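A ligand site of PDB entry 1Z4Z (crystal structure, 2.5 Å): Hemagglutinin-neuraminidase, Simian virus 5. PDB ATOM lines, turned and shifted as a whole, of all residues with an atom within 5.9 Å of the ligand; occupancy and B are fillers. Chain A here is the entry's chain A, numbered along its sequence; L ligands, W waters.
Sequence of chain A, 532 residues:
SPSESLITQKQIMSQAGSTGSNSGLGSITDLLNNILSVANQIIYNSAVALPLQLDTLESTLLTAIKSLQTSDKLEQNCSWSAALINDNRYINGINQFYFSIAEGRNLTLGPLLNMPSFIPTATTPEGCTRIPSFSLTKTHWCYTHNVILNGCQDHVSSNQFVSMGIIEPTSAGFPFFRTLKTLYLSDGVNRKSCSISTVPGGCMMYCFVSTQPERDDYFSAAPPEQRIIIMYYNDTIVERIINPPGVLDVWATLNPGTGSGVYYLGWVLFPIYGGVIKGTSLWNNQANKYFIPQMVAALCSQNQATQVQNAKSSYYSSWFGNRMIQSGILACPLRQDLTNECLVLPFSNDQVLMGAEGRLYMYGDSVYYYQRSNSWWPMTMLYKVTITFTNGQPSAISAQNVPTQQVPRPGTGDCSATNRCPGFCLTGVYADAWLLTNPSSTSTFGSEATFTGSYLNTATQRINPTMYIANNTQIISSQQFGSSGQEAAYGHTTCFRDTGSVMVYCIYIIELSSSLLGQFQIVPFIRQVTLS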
ATOM      1  N   ARG A 130     -24.530  10.088  15.853  1.00  0.00           N
ATOM      2  CA  ARG A 130     -24.702  10.375  14.432  1.00  0.00           C
ATOM      3  C   ARG A 130     -26.114  10.773  14.041  1.00  0.00           C
ATOM      4  O   ARG A 130     -27.039  10.711  14.834  1.00  0.00           O
ATOM      5  CB  ARG A 130     -24.328   9.161  13.578  1.00  0.00           C
ATOM      6  CG  ARG A 130     -22.855   8.909  13.410  1.00  0.00           C
ATOM      7  CD  ARG A 130     -22.639   8.211  12.075  1.00  0.00           C
ATOM      8  NE  ARG A 130     -23.036   9.074  10.976  1.00  0.00           N
ATOM      9  CZ  ARG A 130     -23.187   8.679   9.708  1.00  0.00           C
ATOM     10  NH1 ARG A 130     -22.959   7.409   9.383  1.00  0.00           N
ATOM     11  NH2 ARG A 130     -23.548   9.545   8.782  1.00  0.00           N
ATOM     12  N   ILE A 131     -26.239  11.176  12.775  1.00  0.00           N
ATOM     13  CA  ILE A 131     -27.503  11.580  12.171  1.00  0.00           C
ATOM     14  C   ILE A 131     -28.203  12.719  12.890  1.00  0.00           C
ATOM     15  O   ILE A 131     -29.253  12.537  13.489  1.00  0.00           O
ATOM     16  CB  ILE A 131     -28.476  10.382  12.094  1.00  0.00           C
ATOM     17  CG1 ILE A 131     -27.716   9.128  11.646  1.00  0.00           C
ATOM     18  CG2 ILE A 131     -29.576  10.671  11.085  1.00  0.00           C
ATOM     19  CD1 ILE A 131     -26.956   9.295  10.342  1.00  0.00           C
ATOM     20  N   LYS A 192     -34.852   5.580  14.546  1.00  0.00           N
ATOM     21  CA  LYS A 192     -33.762   5.921  13.629  1.00  0.00           C
ATOM     22  C   LYS A 192     -34.149   6.942  12.571  1.00  0.00           C
ATOM     23  O   LYS A 192     -35.334   7.267  12.400  1.00  0.00           O
ATOM     24  CB  LYS A 192     -33.258   4.674  12.904  1.00  0.00           C
ATOM     25  CG  LYS A 192     -32.612   3.630  13.784  1.00  0.00           C
ATOM     26  CD  LYS A 192     -31.263   4.108  14.300  1.00  0.00           C
ATOM     27  CE  LYS A 192     -30.411   2.918  14.692  1.00  0.00           C
ATOM     28  NZ  LYS A 192     -29.053   3.355  15.112  1.00  0.00           N
ATOM     29  N   SER A 193     -33.135   7.431  11.868  1.00  0.00           N
ATOM     30  CA  SER A 193     -33.309   8.387  10.772  1.00  0.00           C
ATOM     31  C   SER A 193     -34.283   9.507  11.122  1.00  0.00           C
ATOM     32  O   SER A 193     -35.056   9.961  10.277  1.00  0.00           O
ATOM     33  CB  SER A 193     -33.780   7.603   9.536  1.00  0.00           C
ATOM     34  OG  SER A 193     -33.600   8.332   8.332  1.00  0.00           O
ATOM     35  N   PHE A 208     -38.616   6.359  12.572  1.00  0.00           N
ATOM     36  CA  PHE A 208     -39.182   5.081  12.183  1.00  0.00           C
ATOM     37  C   PHE A 208     -38.460   4.125  13.102  1.00  0.00           C
ATOM     38  O   PHE A 208     -37.357   4.446  13.571  1.00  0.00           O
ATOM     39  CB  PHE A 208     -38.927   4.771  10.689  1.00  0.00           C
ATOM     40  CG  PHE A 208     -37.600   4.118  10.386  1.00  0.00           C
ATOM     41  CD1 PHE A 208     -37.460   2.739  10.437  1.00  0.00           C
ATOM     42  CD2 PHE A 208     -36.507   4.889   9.994  1.00  0.00           C
ATOM     43  CE1 PHE A 208     -36.246   2.120  10.091  1.00  0.00           C
ATOM     44  CE2 PHE A 208     -35.285   4.291   9.650  1.00  0.00           C
ATOM     45  CZ  PHE A 208     -35.163   2.901   9.696  1.00  0.00           C
ATOM     46  N   GLU A 214     -31.015  -2.245   7.132  1.00  0.00           N
ATOM     47  CA  GLU A 214     -31.710  -1.417   6.149  1.00  0.00           C
ATOM     48  C   GLU A 214     -32.141  -2.189   4.915  1.00  0.00           C
ATOM     49  O   GLU A 214     -33.290  -2.090   4.479  1.00  0.00           O
ATOM     50  CB  GLU A 214     -30.826  -0.243   5.732  1.00  0.00           C
ATOM     51  CG  GLU A 214     -31.382   0.545   4.555  1.00  0.00           C
ATOM     52  CD  GLU A 214     -30.607   1.813   4.278  1.00  0.00           C
ATOM     53  OE1 GLU A 214     -29.361   1.751   4.269  1.00  0.00           O
ATOM     54  OE2 GLU A 214     -31.241   2.868   4.062  1.00  0.00           O
ATOM     55  N   TYR A 218     -36.159  -3.180   2.719  1.00  0.00           N
ATOM     56  CA  TYR A 218     -36.664  -3.075   1.361  1.00  0.00           C
ATOM     57  C   TYR A 218     -37.253  -4.378   0.819  1.00  0.00           C
ATOM     58  O   TYR A 218     -38.185  -4.354   0.009  1.00  0.00           O
ATOM     59  CB  TYR A 218     -35.560  -2.578   0.419  1.00  0.00           C
ATOM     60  CG  TYR A 218     -35.239  -1.125   0.618  1.00  0.00           C
ATOM     61  CD1 TYR A 218     -34.422  -0.699   1.661  1.00  0.00           C
ATOM     62  CD2 TYR A 218     -35.793  -0.146  -0.213  1.00  0.00           C
ATOM     63  CE1 TYR A 218     -34.174   0.653   1.885  1.00  0.00           C
ATOM     64  CE2 TYR A 218     -35.561   1.208   0.002  1.00  0.00           C
ATOM     65  CZ  TYR A 218     -34.750   1.601   1.060  1.00  0.00           C
ATOM     66  OH  TYR A 218     -34.534   2.936   1.303  1.00  0.00           O
ATOM     67  N   ASN A 255     -38.817   6.151   5.399  1.00  0.00           N
ATOM     68  CA  ASN A 255     -37.871   6.778   6.329  1.00  0.00           C
ATOM     69  C   ASN A 255     -37.960   8.297   6.323  1.00  0.00           C
ATOM     70  O   ASN A 255     -38.251   8.900   5.287  1.00  0.00           O
ATOM     71  CB  ASN A 255     -36.427   6.461   5.927  1.00  0.00           C
ATOM     72  CG  ASN A 255     -36.013   5.047   6.193  1.00  0.00           C
ATOM     73  OD1 ASN A 255     -36.803   4.220   6.651  1.00  0.00           O
ATOM     74  ND2 ASN A 255     -34.756   4.747   5.901  1.00  0.00           N
ATOM     75  N   TYR A 273     -38.343   9.340   2.297  1.00  0.00           N
ATOM     76  CA  TYR A 273     -37.860   8.538   1.190  1.00  0.00           C
ATOM     77  C   TYR A 273     -38.008   7.065   1.551  1.00  0.00           C
ATOM     78  O   TYR A 273     -38.199   6.720   2.718  1.00  0.00           O
ATOM     79  CB  TYR A 273     -36.397   8.883   0.839  1.00  0.00           C
ATOM     80  CG  TYR A 273     -35.342   8.294   1.746  1.00  0.00           C
ATOM     81  CD1 TYR A 273     -35.122   8.801   3.022  1.00  0.00           C
ATOM     82  CD2 TYR A 273     -34.527   7.251   1.294  1.00  0.00           C
ATOM     83  CE1 TYR A 273     -34.106   8.282   3.837  1.00  0.00           C
ATOM     84  CE2 TYR A 273     -33.508   6.722   2.100  1.00  0.00           C
ATOM     85  CZ  TYR A 273     -33.313   7.239   3.364  1.00  0.00           C
ATOM     86  OH  TYR A 273     -32.305   6.726   4.158  1.00  0.00           O
ATOM     87  N   PHE A 320     -31.800  -3.174  -3.383  1.00  0.00           N
ATOM     88  CA  PHE A 320     -32.773  -2.868  -2.344  1.00  0.00           C
ATOM     89  C   PHE A 320     -34.157  -3.424  -2.697  1.00  0.00           C
ATOM     90  O   PHE A 320     -35.073  -2.668  -3.023  1.00  0.00           O
ATOM     91  CB  PHE A 320     -32.868  -1.362  -2.105  1.00  0.00           C
ATOM     92  CG  PHE A 320     -31.851  -0.830  -1.120  1.00  0.00           C
ATOM     93  CD1 PHE A 320     -31.149  -1.687  -0.274  1.00  0.00           C
ATOM     94  CD2 PHE A 320     -31.632   0.536  -1.019  1.00  0.00           C
ATOM     95  CE1 PHE A 320     -30.240  -1.185   0.657  1.00  0.00           C
ATOM     96  CE2 PHE A 320     -30.718   1.045  -0.083  1.00  0.00           C
ATOM     97  CZ  PHE A 320     -30.031   0.191   0.754  1.00  0.00           C
ATOM     98  N   ALA A 356     -33.905   9.866  -1.747  1.00  0.00           N
ATOM     99  CA  ALA A 356     -32.772   9.875  -0.836  1.00  0.00           C
ATOM    100  C   ALA A 356     -33.131  10.690   0.399  1.00  0.00           C
ATOM    101  O   ALA A 356     -34.244  11.230   0.502  1.00  0.00           O
ATOM    102  CB  ALA A 356     -31.551  10.486  -1.523  1.00  0.00           C
ATOM    103  N   GLU A 357     -32.194  10.783   1.346  1.00  0.00           N
ATOM    104  CA  GLU A 357     -32.441  11.574   2.541  1.00  0.00           C
ATOM    105  C   GLU A 357     -32.661  12.990   2.040  1.00  0.00           C
ATOM    106  O   GLU A 357     -32.330  13.309   0.892  1.00  0.00           O
ATOM    107  CB  GLU A 357     -31.234  11.531   3.477  1.00  0.00           C
ATOM    108  CG  GLU A 357     -30.903  10.158   4.028  1.00  0.00           C
ATOM    109  CD  GLU A 357     -29.620  10.175   4.829  1.00  0.00           C
ATOM    110  OE1 GLU A 357     -28.667  10.875   4.398  1.00  0.00           O
ATOM    111  OE2 GLU A 357     -29.532   9.486   5.876  1.00  0.00           O
ATOM    112  N   ARG A 372     -30.565  14.672  -1.037  1.00  0.00           N
ATOM    113  CA  ARG A 372     -29.239  14.072  -1.035  1.00  0.00           C
ATOM    114  C   ARG A 372     -29.012  13.445  -2.406  1.00  0.00           C
ATOM    115  O   ARG A 372     -29.936  12.895  -3.005  1.00  0.00           O
ATOM    116  CB  ARG A 372     -29.143  13.009   0.058  1.00  0.00           C
ATOM    117  CG  ARG A 372     -27.978  12.057  -0.074  1.00  0.00           C
ATOM    118  CD  ARG A 372     -27.856  11.184   1.144  1.00  0.00           C
ATOM    119  NE  ARG A 372     -26.972  10.049   0.914  1.00  0.00           N
ATOM    120  CZ  ARG A 372     -26.536   9.229   1.861  1.00  0.00           C
ATOM    121  NH1 ARG A 372     -26.914   9.416   3.119  1.00  0.00           N
ATOM    122  NH2 ARG A 372     -25.744   8.214   1.560  1.00  0.00           N
ATOM    123  N   ASN A 374     -27.806  10.638  -3.876  1.00  0.00           N
ATOM    124  CA  ASN A 374     -27.414   9.255  -3.634  1.00  0.00           C
ATOM    125  C   ASN A 374     -27.475   8.497  -4.964  1.00  0.00           C
ATOM    126  O   ASN A 374     -27.291   7.281  -5.001  1.00  0.00           O
ATOM    127  CB  ASN A 374     -28.373   8.636  -2.610  1.00  0.00           C
ATOM    128  CG  ASN A 374     -27.690   7.615  -1.719  1.00  0.00           C
ATOM    129  OD1 ASN A 374     -26.564   7.834  -1.267  1.00  0.00           O
ATOM    130  ND2 ASN A 374     -28.365   6.505  -1.456  1.00  0.00           N
ATOM    131  N   LEU A 426     -26.141   4.057  -6.028  1.00  0.00           N
ATOM    132  CA  LEU A 426     -26.687   4.008  -4.688  1.00  0.00           C
ATOM    133  C   LEU A 426     -25.553   4.323  -3.724  1.00  0.00           C
ATOM    134  O   LEU A 426     -25.199   3.517  -2.864  1.00  0.00           O
ATOM    135  CB  LEU A 426     -27.253   2.610  -4.408  1.00  0.00           C
ATOM    136  CG  LEU A 426     -28.142   2.438  -3.174  1.00  0.00           C
ATOM    137  CD1 LEU A 426     -29.347   3.357  -3.275  1.00  0.00           C
ATOM    138  CD2 LEU A 426     -28.585   0.977  -3.078  1.00  0.00           C
ATOM    139  N   GLY A 428     -23.276   7.943  -1.800  1.00  0.00           N
ATOM    140  CA  GLY A 428     -23.201   9.375  -1.560  1.00  0.00           C
ATOM    141  C   GLY A 428     -23.183   9.739  -0.076  1.00  0.00           C
ATOM    142  O   GLY A 428     -22.930   8.897   0.775  1.00  0.00           O
ATOM    143  N   VAL A 429     -23.433  11.015   0.220  1.00  0.00           N
ATOM    144  CA  VAL A 429     -23.473  11.511   1.598  1.00  0.00           C
ATOM    145  C   VAL A 429     -24.440  12.669   1.685  1.00  0.00           C
ATOM    146  O   VAL A 429     -24.710  13.343   0.686  1.00  0.00           O
ATOM    147  CB  VAL A 429     -22.131  12.090   2.091  1.00  0.00           C
ATOM    148  CG1 VAL A 429     -21.705  11.397   3.364  1.00  0.00           C
ATOM    149  CG2 VAL A 429     -21.079  12.015   1.008  1.00  0.00           C
ATOM    150  N   ARG A 462     -15.006   9.684   2.292  1.00  0.00           N
ATOM    151  CA  ARG A 462     -15.678  10.664   3.126  1.00  0.00           C
ATOM    152  C   ARG A 462     -14.557  11.345   3.912  1.00  0.00           C
ATOM    153  O   ARG A 462     -14.318  11.046   5.085  1.00  0.00           O
ATOM    154  CB  ARG A 462     -16.677   9.970   4.052  1.00  0.00           C
ATOM    155  CG  ARG A 462     -17.879   9.433   3.299  1.00  0.00           C
ATOM    156  CD  ARG A 462     -18.975   8.987   4.239  1.00  0.00           C
ATOM    157  NE  ARG A 462     -20.202   8.646   3.524  1.00  0.00           N
ATOM    158  CZ  ARG A 462     -21.329   8.278   4.112  1.00  0.00           C
ATOM    159  NH1 ARG A 462     -21.386   8.203   5.444  1.00  0.00           N
ATOM    160  NH2 ARG A 462     -22.392   7.987   3.380  1.00  0.00           N
ATOM    161  N   ALA A 489     -18.554  13.069   7.885  1.00  0.00           N
ATOM    162  CA  ALA A 489     -19.706  12.469   7.241  1.00  0.00           C
ATOM    163  C   ALA A 489     -20.744  13.518   6.842  1.00  0.00           C
ATOM    164  O   ALA A 489     -20.471  14.334   5.963  1.00  0.00           O
ATOM    165  CB  ALA A 489     -20.317  11.399   8.154  1.00  0.00           C
ATOM    166  N   TYR A 490     -21.920  13.503   7.462  1.00  0.00           N
ATOM    167  CA  TYR A 490     -22.991  14.454   7.146  1.00  0.00           C
ATOM    168  C   TYR A 490     -22.681  15.896   7.528  1.00  0.00           C
ATOM    169  O   TYR A 490     -21.852  16.158   8.408  1.00  0.00           O
ATOM    170  CB  TYR A 490     -24.305  14.055   7.833  1.00  0.00           C
ATOM    171  CG  TYR A 490     -24.951  12.787   7.341  1.00  0.00           C
ATOM    172  CD1 TYR A 490     -24.291  11.927   6.460  1.00  0.00           C
ATOM    173  CD2 TYR A 490     -26.242  12.450   7.753  1.00  0.00           C
ATOM    174  CE1 TYR A 490     -24.902  10.759   6.010  1.00  0.00           C
ATOM    175  CE2 TYR A 490     -26.855  11.288   7.295  1.00  0.00           C
ATOM    176  CZ  TYR A 490     -26.180  10.449   6.428  1.00  0.00           C
ATOM    177  OH  TYR A 490     -26.817   9.322   5.964  1.00  0.00           O
HETATM  178  C1  LIG L   1     -24.863   6.990   5.599  1.00  0.00           C
HETATM  179  C2  LIG L   1     -26.139   6.548   6.031  1.00  0.00           C
HETATM  180  C3  LIG L   1     -26.468   6.540   7.526  1.00  0.00           C
HETATM  181  C4  LIG L   1     -27.972   6.343   7.793  1.00  0.00           C
HETATM  182  C5  LIG L   1     -28.597   5.425   6.763  1.00  0.00           C
HETATM  183  C6  LIG L   1     -28.390   6.068   5.362  1.00  0.00           C
HETATM  184  C7  LIG L   1     -28.954   5.185   4.233  1.00  0.00           C
HETATM  185  C8  LIG L   1     -28.815   5.831   2.860  1.00  0.00           C
HETATM  186  C9  LIG L   1     -29.385   4.915   1.745  1.00  0.00           C
HETATM  187  C10 LIG L   1     -30.602   4.144   7.368  1.00  0.00           C
HETATM  188  C11 LIG L   1     -32.074   4.149   7.691  1.00  0.00           C
HETATM  189  N1  LIG L   1     -30.013   5.295   7.089  1.00  0.00           N
HETATM  190  O1  LIG L   1     -23.839   7.293   6.461  1.00  0.00           O
HETATM  191  O2  LIG L   1     -24.656   7.126   4.311  1.00  0.00           O
HETATM  192  O3  LIG L   1     -28.124   5.799   9.106  1.00  0.00           O
HETATM  193  O4  LIG L   1     -26.984   6.198   5.114  1.00  0.00           O
HETATM  194  O5  LIG L   1     -28.226   3.960   4.166  1.00  0.00           O
HETATM  195  O6  LIG L   1     -29.542   7.066   2.846  1.00  0.00           O
HETATM  196  O7  LIG L   1     -30.732   4.552   1.934  1.00  0.00           O
HETATM  197  O8  LIG L   1     -29.930   2.941   7.390  1.00  0.00           O
HETATM  198  O   HOH W   1     -31.516   7.754   6.569  1.00  0.00           O
HETATM  199  O   HOH W   2     -30.283   8.710   0.678  1.00  0.00           O
HETATM  200  O   HOH W   3     -31.145   1.264   9.400  1.00  0.00           O
HETATM  201  O   HOH W   4     -30.643   6.555  10.122  1.00  0.00           O
HETATM  202  O   HOH W   5     -32.391   4.618  -0.329  1.00  0.00           O
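The side-chain carboxylate (OE1) of Glu 214 lies within hydrogen-bond range of an oxygen (O5) of the ligand, at 2.5 Å. NH2 of Arg 462 is in salt-bridge range of O2 of the ligand (2.6 Å). The side-chain hydroxyl (OH) of Tyr 490 lies close to an oxygen (O4) of the ligand (3.2 Å). NH1 of Arg 130 lies within salt-bridge range of O1 of the ligand. The side-chain hydroxyl (OH) of Tyr 273 lies within hydrogen-bond range of an oxygen (O6) of the ligand. NH2 of Arg 372 is in salt-bridge range of O2 of the ligand, at 3.2 Å.
The guanidinium group (NH2) of Arg 462 is in hydrogen-bond range of the backbone carbonyl oxygen (O) of Gly 428 (2.8 Å). The guanidinium group (NH1) of Arg 372 is in hydrogen-bond range of the side-chain hydroxyl (OH) of Tyr 490, 2.8 Å away. OE2 of Glu 357 lies within hydrogen-bond range of OH of Tyr 490. The backbone carbonyl oxygen of Tyr 273 sits at hydrogen-bond distance from the backbone NH of Asn 255, at 2.8 Å. The side-chain carboxylate of Glu 357 is in salt-bridge range of the guanidinium group of Arg 372 (2.6 Å). OD1 of Asn 374 is in hydrogen-bond range of NH2 of Arg 372 (3.0 Å). N of Gly 428 is in hydrogen-bond range of OD1 of Asn 374 (3.3 Å). The backbone carbonyl oxygen (O) of Phe 208 is in hydrogen-bond range of the backbone NH (N) of Lys 192 (2.9 Å).
Water W5 lies within hydrogen-bond range of O7 of the ligand (2.8 Å) and OH of Tyr 218 (3.2 Å). Water W4 bridges O3 of the ligand (2.8 Å) and N of Ser 193 (3.2 Å). Water W2 bridges an oxygen (O6) of the ligand (2.8 Å) and the backbone NH (N) of Glu 357 (2.9 Å). Water W1 lies within hydrogen-bond range of the side-chain carboxylate of Glu 357 (2.7 Å), the side-chain hydroxyl of Tyr 273 (2.7 Å), the side-chain hydroxyl of Ser 193 (2.8 Å) and a nitrogen (N1) of the ligand (2.9 Å).
Residues that only touch the ligand: Asn 255 (3.3 Å), Glu 357 (3.6 Å), Asn 374 (3.7 Å), Phe 208 (3.8 Å) and Ile 131 (3.9 Å). Hydrophobic or aromatic side chains within 4 Å of the ligand: Ile 131, Phe 208, Tyr 273 and Tyr 490. Of the 20 residues printed, 11 come within 4 Å of the ligand.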
